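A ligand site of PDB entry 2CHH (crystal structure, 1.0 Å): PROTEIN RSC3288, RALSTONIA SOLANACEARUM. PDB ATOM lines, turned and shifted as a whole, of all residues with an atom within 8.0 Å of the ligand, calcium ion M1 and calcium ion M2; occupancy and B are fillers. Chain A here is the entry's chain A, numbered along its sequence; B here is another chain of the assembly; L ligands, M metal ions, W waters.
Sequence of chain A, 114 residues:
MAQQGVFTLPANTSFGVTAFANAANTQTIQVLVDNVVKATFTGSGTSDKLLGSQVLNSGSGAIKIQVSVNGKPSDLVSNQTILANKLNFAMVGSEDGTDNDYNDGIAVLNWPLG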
ATOM      1  N   ALA A  21      11.553   2.979  34.095  1.00  0.00           N
ATOM      2  CA  ALA A  21      12.262   2.363  32.980  1.00  0.00           C
ATOM      3  C   ALA A  21      11.392   1.374  32.267  1.00  0.00           C
ATOM      4  O   ALA A  21      10.612   0.637  32.853  1.00  0.00           O
ATOM      5  CB  ALA A  21      13.530   1.678  33.440  1.00  0.00           C
ATOM      6  N   ASN A  22      11.603   1.320  30.945  1.00  0.00           N
ATOM      7  CA  ASN A  22      11.119   0.218  30.087  1.00  0.00           C
ATOM      8  C   ASN A  22      12.246  -0.088  29.130  1.00  0.00           C
ATOM      9  O   ASN A  22      12.215   0.303  27.947  1.00  0.00           O
ATOM     10  CB  ASN A  22       9.853   0.577  29.323  1.00  0.00           C
ATOM     11  CG  ASN A  22       8.692   0.787  30.215  1.00  0.00           C
ATOM     12  OD1 ASN A  22       8.023  -0.165  30.601  1.00  0.00           O
ATOM     13  ND2 ASN A  22       8.426   2.042  30.550  1.00  0.00           N
ATOM     14  N   ALA A  23      13.300  -0.710  29.612  1.00  0.00           N
ATOM     15  CA  ALA A  23      14.569  -0.763  28.886  1.00  0.00           C
ATOM     16  C   ALA A  23      15.435  -1.848  29.462  1.00  0.00           C
ATOM     17  O   ALA A  23      15.445  -2.091  30.670  1.00  0.00           O
ATOM     18  CB  ALA A  23      15.305   0.559  29.026  1.00  0.00           C
ATOM     19  N   ALA A  24      16.230  -2.468  28.581  1.00  0.00           N
ATOM     20  CA  ALA A  24      17.282  -3.385  29.037  1.00  0.00           C
ATOM     21  C   ALA A  24      18.467  -2.626  29.596  1.00  0.00           C
ATOM     22  O   ALA A  24      19.161  -3.095  30.492  1.00  0.00           O
ATOM     23  CB  ALA A  24      17.704  -4.277  27.908  1.00  0.00           C
ATOM     24  N   ASN A  25      18.757  -1.442  29.063  1.00  0.00           N
ATOM     25  CA  ASN A  25      19.902  -0.649  29.520  1.00  0.00           C
ATOM     26  C   ASN A  25      19.544   0.179  30.729  1.00  0.00           C
ATOM     27  O   ASN A  25      18.388   0.631  30.885  1.00  0.00           O
ATOM     28  CB  ASN A  25      20.445   0.187  28.406  1.00  0.00           C
ATOM     29  CG  ASN A  25      21.180  -0.691  27.341  1.00  0.00           C
ATOM     30  OD1 ASN A  25      21.672  -1.787  27.713  1.00  0.00           O
ATOM     31  ND2 ASN A  25      21.355  -0.199  26.166  1.00  0.00           N
ATOM     32  N   THR A  26      20.541   0.443  31.561  1.00  0.00           N
ATOM     33  CA  THR A  26      20.347   1.252  32.739  1.00  0.00           C
ATOM     34  C   THR A  26      20.116   2.710  32.350  1.00  0.00           C
ATOM     35  O   THR A  26      20.961   3.324  31.695  1.00  0.00           O
ATOM     36  CB  THR A  26      21.579   1.161  33.635  1.00  0.00           C
ATOM     37  OG1 THR A  26      21.782  -0.209  33.969  1.00  0.00           O
ATOM     38  CG2 THR A  26      21.413   1.966  34.889  1.00  0.00           C
ATOM     39  N   GLN A  27      18.989   3.222  32.802  1.00  0.00           N
ATOM     40  CA  GLN A  27      18.613   4.609  32.568  1.00  0.00           C
ATOM     41  C   GLN A  27      19.113   5.466  33.721  1.00  0.00           C
ATOM     42  O   GLN A  27      19.023   5.063  34.865  1.00  0.00           O
ATOM     43  CB  GLN A  27      17.088   4.699  32.530  1.00  0.00           C
ATOM     44  CG  GLN A  27      16.437   3.732  31.521  1.00  0.00           C
ATOM     45  CD  GLN A  27      16.815   4.039  30.107  1.00  0.00           C
ATOM     46  OE1 GLN A  27      16.561   5.149  29.651  1.00  0.00           O
ATOM     47  NE2 GLN A  27      17.385   3.076  29.400  1.00  0.00           N
ATOM     48  N   SER A  44      16.908  -0.143  35.462  1.00  0.00           N
ATOM     49  CA  SER A  44      16.502  -0.803  34.229  1.00  0.00           C
ATOM     50  C   SER A  44      15.365  -1.738  34.533  1.00  0.00           C
ATOM     51  O   SER A  44      15.031  -1.990  35.683  1.00  0.00           O
ATOM     52  CB  SER A  44      17.649  -1.563  33.575  1.00  0.00           C
ATOM     53  OG  SER A  44      18.086  -2.611  34.410  1.00  0.00           O
ATOM     54  N   GLY A  45      14.787  -2.291  33.492  1.00  0.00           N
ATOM     55  CA  GLY A  45      13.679  -3.223  33.611  1.00  0.00           C
ATOM     56  C   GLY A  45      12.697  -2.881  32.502  1.00  0.00           C
ATOM     57  O   GLY A  45      12.541  -1.717  32.129  1.00  0.00           O
ATOM     58  N   THR A  46      12.036  -3.910  32.001  1.00  0.00           N
ATOM     59  CA  THR A  46      11.193  -3.730  30.812  1.00  0.00           C
ATOM     60  C   THR A  46       9.689  -3.690  31.100  1.00  0.00           C
ATOM     61  O   THR A  46       8.919  -3.570  30.165  1.00  0.00           O
ATOM     62  CB  THR A  46      11.507  -4.777  29.760  1.00  0.00           C
ATOM     63  OG1 THR A  46      11.341  -6.060  30.359  1.00  0.00           O
ATOM     64  CG2 THR A  46      12.942  -4.645  29.271  1.00  0.00           C
ATOM     65  N   SER A  47       9.298  -3.750  32.379  1.00  0.00           N
ATOM     66  CA  SER A  47       7.884  -3.730  32.821  1.00  0.00           C
ATOM     67  C   SER A  47       7.583  -2.516  33.679  1.00  0.00           C
ATOM     68  O   SER A  47       7.157  -2.619  34.824  1.00  0.00           O
ATOM     69  CB  SER A  47       7.533  -5.017  33.564  1.00  0.00           C
ATOM     70  OG  SER A  47       7.550  -6.082  32.611  1.00  0.00           O
ATOM     71  N   VAL A  69      22.071   7.052  29.046  1.00  0.00           N
ATOM     72  CA  VAL A  69      22.471   5.680  29.304  1.00  0.00           C
ATOM     73  C   VAL A  69      24.006   5.719  29.298  1.00  0.00           C
ATOM     74  O   VAL A  69      24.624   6.000  28.264  1.00  0.00           O
ATOM     75  CB  VAL A  69      21.958   4.716  28.281  1.00  0.00           C
ATOM     76  CG1 VAL A  69      22.587   3.320  28.525  1.00  0.00           C
ATOM     77  CG2 VAL A  69      20.480   4.681  28.354  1.00  0.00           C
ATOM     78  N   SER A  94      11.686   8.887  26.322  1.00  0.00           N
ATOM     79  CA  SER A  94      13.035   8.923  25.753  1.00  0.00           C
ATOM     80  C   SER A  94      13.304   7.616  25.031  1.00  0.00           C
ATOM     81  O   SER A  94      12.774   6.561  25.379  1.00  0.00           O
ATOM     82  CB  SER A  94      14.059   9.169  26.811  1.00  0.00           C
ATOM     83  OG  SER A  94      14.147   8.101  27.756  1.00  0.00           O
ATOM     84  N   GLU A  95      14.201   7.719  24.060  1.00  0.00           N
ATOM     85  CA  GLU A  95      14.628   6.606  23.250  1.00  0.00           C
ATOM     86  C   GLU A  95      16.147   6.497  23.345  1.00  0.00           C
ATOM     87  O   GLU A  95      16.866   7.451  23.014  1.00  0.00           O
ATOM     88  CB  GLU A  95      14.195   6.764  21.808  1.00  0.00           C
ATOM     89  CG  GLU A  95      14.650   5.627  20.901  1.00  0.00           C
ATOM     90  CD  GLU A  95      14.212   4.287  21.409  1.00  0.00           C
ATOM     91  OE1 GLU A  95      13.019   4.107  21.754  1.00  0.00           O
ATOM     92  OE2 GLU A  95      15.079   3.359  21.524  1.00  0.00           O
ATOM     93  N   ASP A  96      16.618   5.322  23.763  1.00  0.00           N
ATOM     94  CA  ASP A  96      18.037   5.050  23.924  1.00  0.00           C
ATOM     95  C   ASP A  96      18.617   4.216  22.798  1.00  0.00           C
ATOM     96  O   ASP A  96      19.828   3.933  22.816  1.00  0.00           O
ATOM     97  CB  ASP A  96      18.303   4.383  25.282  1.00  0.00           C
ATOM     98  CG  ASP A  96      17.773   2.977  25.390  1.00  0.00           C
ATOM     99  OD1 ASP A  96      17.425   2.386  24.338  1.00  0.00           O
ATOM    100  OD2 ASP A  96      17.720   2.452  26.520  1.00  0.00           O
ATOM    101  N   GLY A  97      17.828   3.876  21.805  1.00  0.00           N
ATOM    102  CA  GLY A  97      18.215   2.896  20.805  1.00  0.00           C
ATOM    103  C   GLY A  97      17.566   3.115  19.491  1.00  0.00           C
ATOM    104  O   GLY A  97      17.533   4.248  19.006  1.00  0.00           O
ATOM    105  N   THR A  98      17.094   2.047  18.878  1.00  0.00           N
ATOM    106  CA  THR A  98      16.626   2.022  17.523  1.00  0.00           C
ATOM    107  C   THR A  98      15.168   1.622  17.350  1.00  0.00           C
ATOM    108  O   THR A  98      14.656   1.767  16.260  1.00  0.00           O
ATOM    109  CB  THR A  98      17.501   1.103  16.665  1.00  0.00           C
ATOM    110  OG1 THR A  98      17.413  -0.191  17.243  1.00  0.00           O
ATOM    111  CG2 THR A  98      18.941   1.571  16.603  1.00  0.00           C
ATOM    112  N   ASP A  99      14.501   1.111  18.376  1.00  0.00           N
ATOM    113  CA  ASP A  99      13.147   0.618  18.188  1.00  0.00           C
ATOM    114  C   ASP A  99      12.096   1.730  18.261  1.00  0.00           C
ATOM    115  O   ASP A  99      10.956   1.499  17.900  1.00  0.00           O
ATOM    116  CB  ASP A  99      12.799  -0.525  19.115  1.00  0.00           C
ATOM    117  CG  ASP A  99      12.722  -0.159  20.568  1.00  0.00           C
ATOM    118  OD1 ASP A  99      13.141   0.953  20.945  1.00  0.00           O
ATOM    119  OD2 ASP A  99      12.287  -1.024  21.366  1.00  0.00           O
ATOM    120  N   ASN A 100      12.460   2.912  18.730  1.00  0.00           N
ATOM    121  CA  ASN A 100      11.569   4.072  18.742  1.00  0.00           C
ATOM    122  C   ASN A 100      10.277   3.822  19.488  1.00  0.00           C
ATOM    123  O   ASN A 100       9.218   4.352  19.129  1.00  0.00           O
ATOM    124  CB  ASN A 100      11.347   4.561  17.339  1.00  0.00           C
ATOM    125  CG  ASN A 100      12.608   5.099  16.751  1.00  0.00           C
ATOM    126  OD1 ASN A 100      13.575   5.445  17.456  1.00  0.00           O
ATOM    127  ND2 ASN A 100      12.672   5.114  15.447  1.00  0.00           N
ATOM    128  N   ASP A 101      10.400   3.165  20.632  1.00  0.00           N
ATOM    129  CA  ASP A 101       9.243   3.026  21.510  1.00  0.00           C
ATOM    130  C   ASP A 101       9.164   4.210  22.473  1.00  0.00           C
ATOM    131  O   ASP A 101       8.083   4.452  23.040  1.00  0.00           O
ATOM    132  CB  ASP A 101       9.208   1.657  22.192  1.00  0.00           C
ATOM    133  CG  ASP A 101      10.339   1.308  23.153  1.00  0.00           C
ATOM    134  OD1 ASP A 101      11.309   2.087  23.248  1.00  0.00           O
ATOM    135  OD2 ASP A 101      10.227   0.237  23.771  1.00  0.00           O
ATOM    136  N   TYR A 102      10.242   4.970  22.648  1.00  0.00           N
ATOM    137  CA  TYR A 102      10.229   6.213  23.433  1.00  0.00           C
ATOM    138  C   TYR A 102       9.784   6.020  24.870  1.00  0.00           C
ATOM    139  O   TYR A 102       9.425   6.984  25.550  1.00  0.00           O
ATOM    140  CB  TYR A 102       9.462   7.347  22.722  1.00  0.00           C
ATOM    141  CG  TYR A 102      10.336   7.961  21.639  1.00  0.00           C
ATOM    142  CD1 TYR A 102      10.409   7.450  20.376  1.00  0.00           C
ATOM    143  CD2 TYR A 102      11.218   8.983  21.955  1.00  0.00           C
ATOM    144  CE1 TYR A 102      11.311   7.961  19.458  1.00  0.00           C
ATOM    145  CE2 TYR A 102      12.128   9.494  21.033  1.00  0.00           C
ATOM    146  CZ  TYR A 102      12.178   8.953  19.814  1.00  0.00           C
ATOM    147  OH  TYR A 102      13.120   9.376  18.864  1.00  0.00           O
ATOM    148  N   ASN A 103       9.914   4.802  25.391  1.00  0.00           N
ATOM    149  CA  ASN A 103       9.484   4.508  26.747  1.00  0.00           C
ATOM    150  C   ASN A 103      10.644   4.133  27.634  1.00  0.00           C
ATOM    151  O   ASN A 103      10.430   3.660  28.776  1.00  0.00           O
ATOM    152  CB  ASN A 103       8.412   3.422  26.762  1.00  0.00           C
ATOM    153  CG  ASN A 103       8.956   2.102  26.357  1.00  0.00           C
ATOM    154  OD1 ASN A 103      10.181   1.974  26.160  1.00  0.00           O
ATOM    155  ND2 ASN A 103       8.119   1.083  26.260  1.00  0.00           N
ATOM    156  N   ASP A 104      11.885   4.312  27.183  1.00  0.00           N
ATOM    157  CA  ASP A 104      13.012   3.657  27.830  1.00  0.00           C
ATOM    158  C   ASP A 104      13.253   4.202  29.224  1.00  0.00           C
ATOM    159  O   ASP A 104      13.456   3.457  30.171  1.00  0.00           O
ATOM    160  CB  ASP A 104      14.229   3.740  26.936  1.00  0.00           C
ATOM    161  CG  ASP A 104      14.024   3.060  25.613  1.00  0.00           C
ATOM    162  OD1 ASP A 104      13.369   1.985  25.543  1.00  0.00           O
ATOM    163  OD2 ASP A 104      14.536   3.567  24.571  1.00  0.00           O
ATOM    164  N   GLY A 105      13.236   5.545  29.297  1.00  0.00           N
ATOM    165  CA  GLY A 105      13.305   6.282  30.529  1.00  0.00           C
ATOM    166  C   GLY A 105      12.210   7.326  30.495  1.00  0.00           C
ATOM    167  O   GLY A 105      12.160   8.139  29.559  1.00  0.00           O
ATOM    168  N   PRO B 112       2.921   1.819  25.425  1.00  0.00           N
ATOM    169  CA  PRO B 112       3.313   0.444  25.712  1.00  0.00           C
ATOM    170  C   PRO B 112       4.531   0.373  26.601  1.00  0.00           C
ATOM    171  O   PRO B 112       5.292   1.314  26.748  1.00  0.00           O
ATOM    172  CB  PRO B 112       3.629  -0.131  24.333  1.00  0.00           C
ATOM    173  CG  PRO B 112       4.171   1.030  23.587  1.00  0.00           C
ATOM    174  CD  PRO B 112       3.355   2.238  24.077  1.00  0.00           C
ATOM    175  N   LEU B 113       4.686  -0.786  27.193  1.00  0.00           N
ATOM    176  CA  LEU B 113       5.850  -1.139  28.000  1.00  0.00           C
ATOM    177  C   LEU B 113       6.868  -1.836  27.136  1.00  0.00           C
ATOM    178  O   LEU B 113       6.750  -1.851  25.917  1.00  0.00           O
ATOM    179  CB  LEU B 113       5.419  -1.929  29.224  1.00  0.00           C
ATOM    180  CG  LEU B 113       4.278  -1.300  30.021  1.00  0.00           C
ATOM    181  CD1 LEU B 113       3.999  -2.131  31.258  1.00  0.00           C
ATOM    182  CD2 LEU B 113       4.553   0.149  30.382  1.00  0.00           C
ATOM    183  N   GLY B 114       7.894  -2.423  27.738  1.00  0.00           N
ATOM    184  CA  GLY B 114       8.881  -3.226  27.013  1.00  0.00           C
ATOM    185  C   GLY B 114      10.135  -2.472  26.652  1.00  0.00           C
ATOM    186  O   GLY B 114      10.101  -1.272  26.363  1.00  0.00           O
ATOM    187  OXT GLY B 114      11.176  -3.178  26.625  1.00  0.00           O
HETATM  188  C1  LIG L   1      14.968  -3.148  25.166  1.00  0.00           C
HETATM  189  C2  LIG L   1      13.781  -2.301  24.755  1.00  0.00           C
HETATM  190  C3  LIG L   1      14.228  -1.163  23.868  1.00  0.00           C
HETATM  191  C4  LIG L   1      15.382  -0.387  24.455  1.00  0.00           C
HETATM  192  C5  LIG L   1      16.541  -1.358  24.724  1.00  0.00           C
HETATM  193  C6  LIG L   1      17.757  -0.763  25.323  1.00  0.00           C
HETATM  194  O1  LIG L   1      15.328  -3.922  24.049  1.00  0.00           O
HETATM  195  O2  LIG L   1      13.189  -1.714  25.923  1.00  0.00           O
HETATM  196  O3  LIG L   1      13.116  -0.279  23.646  1.00  0.00           O
HETATM  197  O4  LIG L   1      15.723   0.622  23.516  1.00  0.00           O
HETATM  198  O5  LIG L   1      16.054  -2.372  25.641  1.00  0.00           O
HETATM  199  O6  LIG L   1      17.500  -0.194  26.600  1.00  0.00           O
HETATM  200 CA    CA M   1      11.748   0.306  25.649  1.00  0.00          CA
HETATM  201 CA    CA M   2      13.666   2.047  22.938  1.00  0.00          CA
HETATM  202  O   HOH W   1      16.291  -0.021  20.717  1.00  0.00           O
HETATM  203  O   HOH W   2      17.339  -5.593  24.230  1.00  0.00           O
HETATM  204  O   HOH W   3      14.912  -4.329  21.281  1.00  0.00           O
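The side-chain carboxylate (OD2) of Asp 96 lies within hydrogen-bond range of an oxygen (O6) of the ligand (2.7 Å). N of Ala 24 is in hydrogen-bond range of O5 of the ligand (2.9 Å). The backbone NH of Asn 25 is in hydrogen-bond range of an oxygen (O6) of the ligand (3.0 Å).
O of Ser 94 is in hydrogen-bond range of N of Asn 103, at 3.4 Å. The backbone carbonyl oxygen of Leu 113 of chain B sits at hydrogen-bond distance from the side-chain amide nitrogen of Asn 103, 3.3 Å away. The side-chain amide nitrogen (NE2) of Gln 27 is in hydrogen-bond range of the side-chain carboxylate (OD2) of Asp 96. The side-chain carboxylate (OD2) of Asp 104 lies close to the backbone NH (N) of Asp 96. N of Asp 104 is in hydrogen-bond range of O of Ser 94, 3.0 Å away. The backbone carbonyl oxygen (O) of Asn 25 sits at hydrogen-bond distance from the side-chain amide nitrogen (NE2) of Gln 27, at 3.0 Å. The backbone NH of Gly 97 lies close to the side-chain carboxylate of Glu 95. N of Gly 114 of chain B lies within hydrogen-bond range of O of Thr 46 (2.9 Å).
Ala 23 touches the ligand (CB to O6, 3.4 Å). Along chain A the residues within 4 Å of the ligand span positions 22 to 104.
Five residues have an atom within 4 Å of calcium ion M1: Asn 22, Asp 101, Asn 103, Asp 104 and Gly 114 of chain B. The nearest printed residue that does not touch calcium ion M1 is Ala 23 (4.4 Å).
Of the 27 residues printed, 4 come within 4 Å of calcium ion M2. Along chain A the residues within 4 Å of calcium ion M2 span positions 95 to 104.
Calcium ion M1 is bound by the side-chain carboxylate of Asp 104 (2.3 Å), the backbone carbonyl oxygen of Asn 22 (2.3 Å), the side-chain amide oxygen of Asn 103 (2.3 Å), the chain-end carboxylate of Gly 114 of chain B (2.4 Å), the side-chain carboxylate of Asp 101 (2.4 Å), an oxygen (O3) of the ligand (2.5 Å) and an oxygen (O2) of the ligand (2.5 Å). Calcium ion M1 has seven donor atoms within binding distance. Slightly farther from calcium ion M1 lies the side-chain carboxylate (OD1) of Asp 101 (3.0 Å).
Calcium ion M2 is bound by the side-chain carboxylate (OD1) of Asp 99 (2.3 Å), the side-chain carboxylate (OD1) of Asp 101 (2.4 Å), the side-chain carboxylate (OE2) of Glu 95 (2.4 Å), the side-chain carboxylate (OD2) of Asp 104 (2.4 Å), the side-chain carboxylate (OE1) of Glu 95 (2.5 Å), an oxygen (O3) of the ligand (2.5 Å), an oxygen (O4) of the ligand (2.6 Å) and the side-chain carboxylate (OD1) of Asp 104 (2.6 Å). Calcium ion M2 has eight donor atoms within binding distance.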
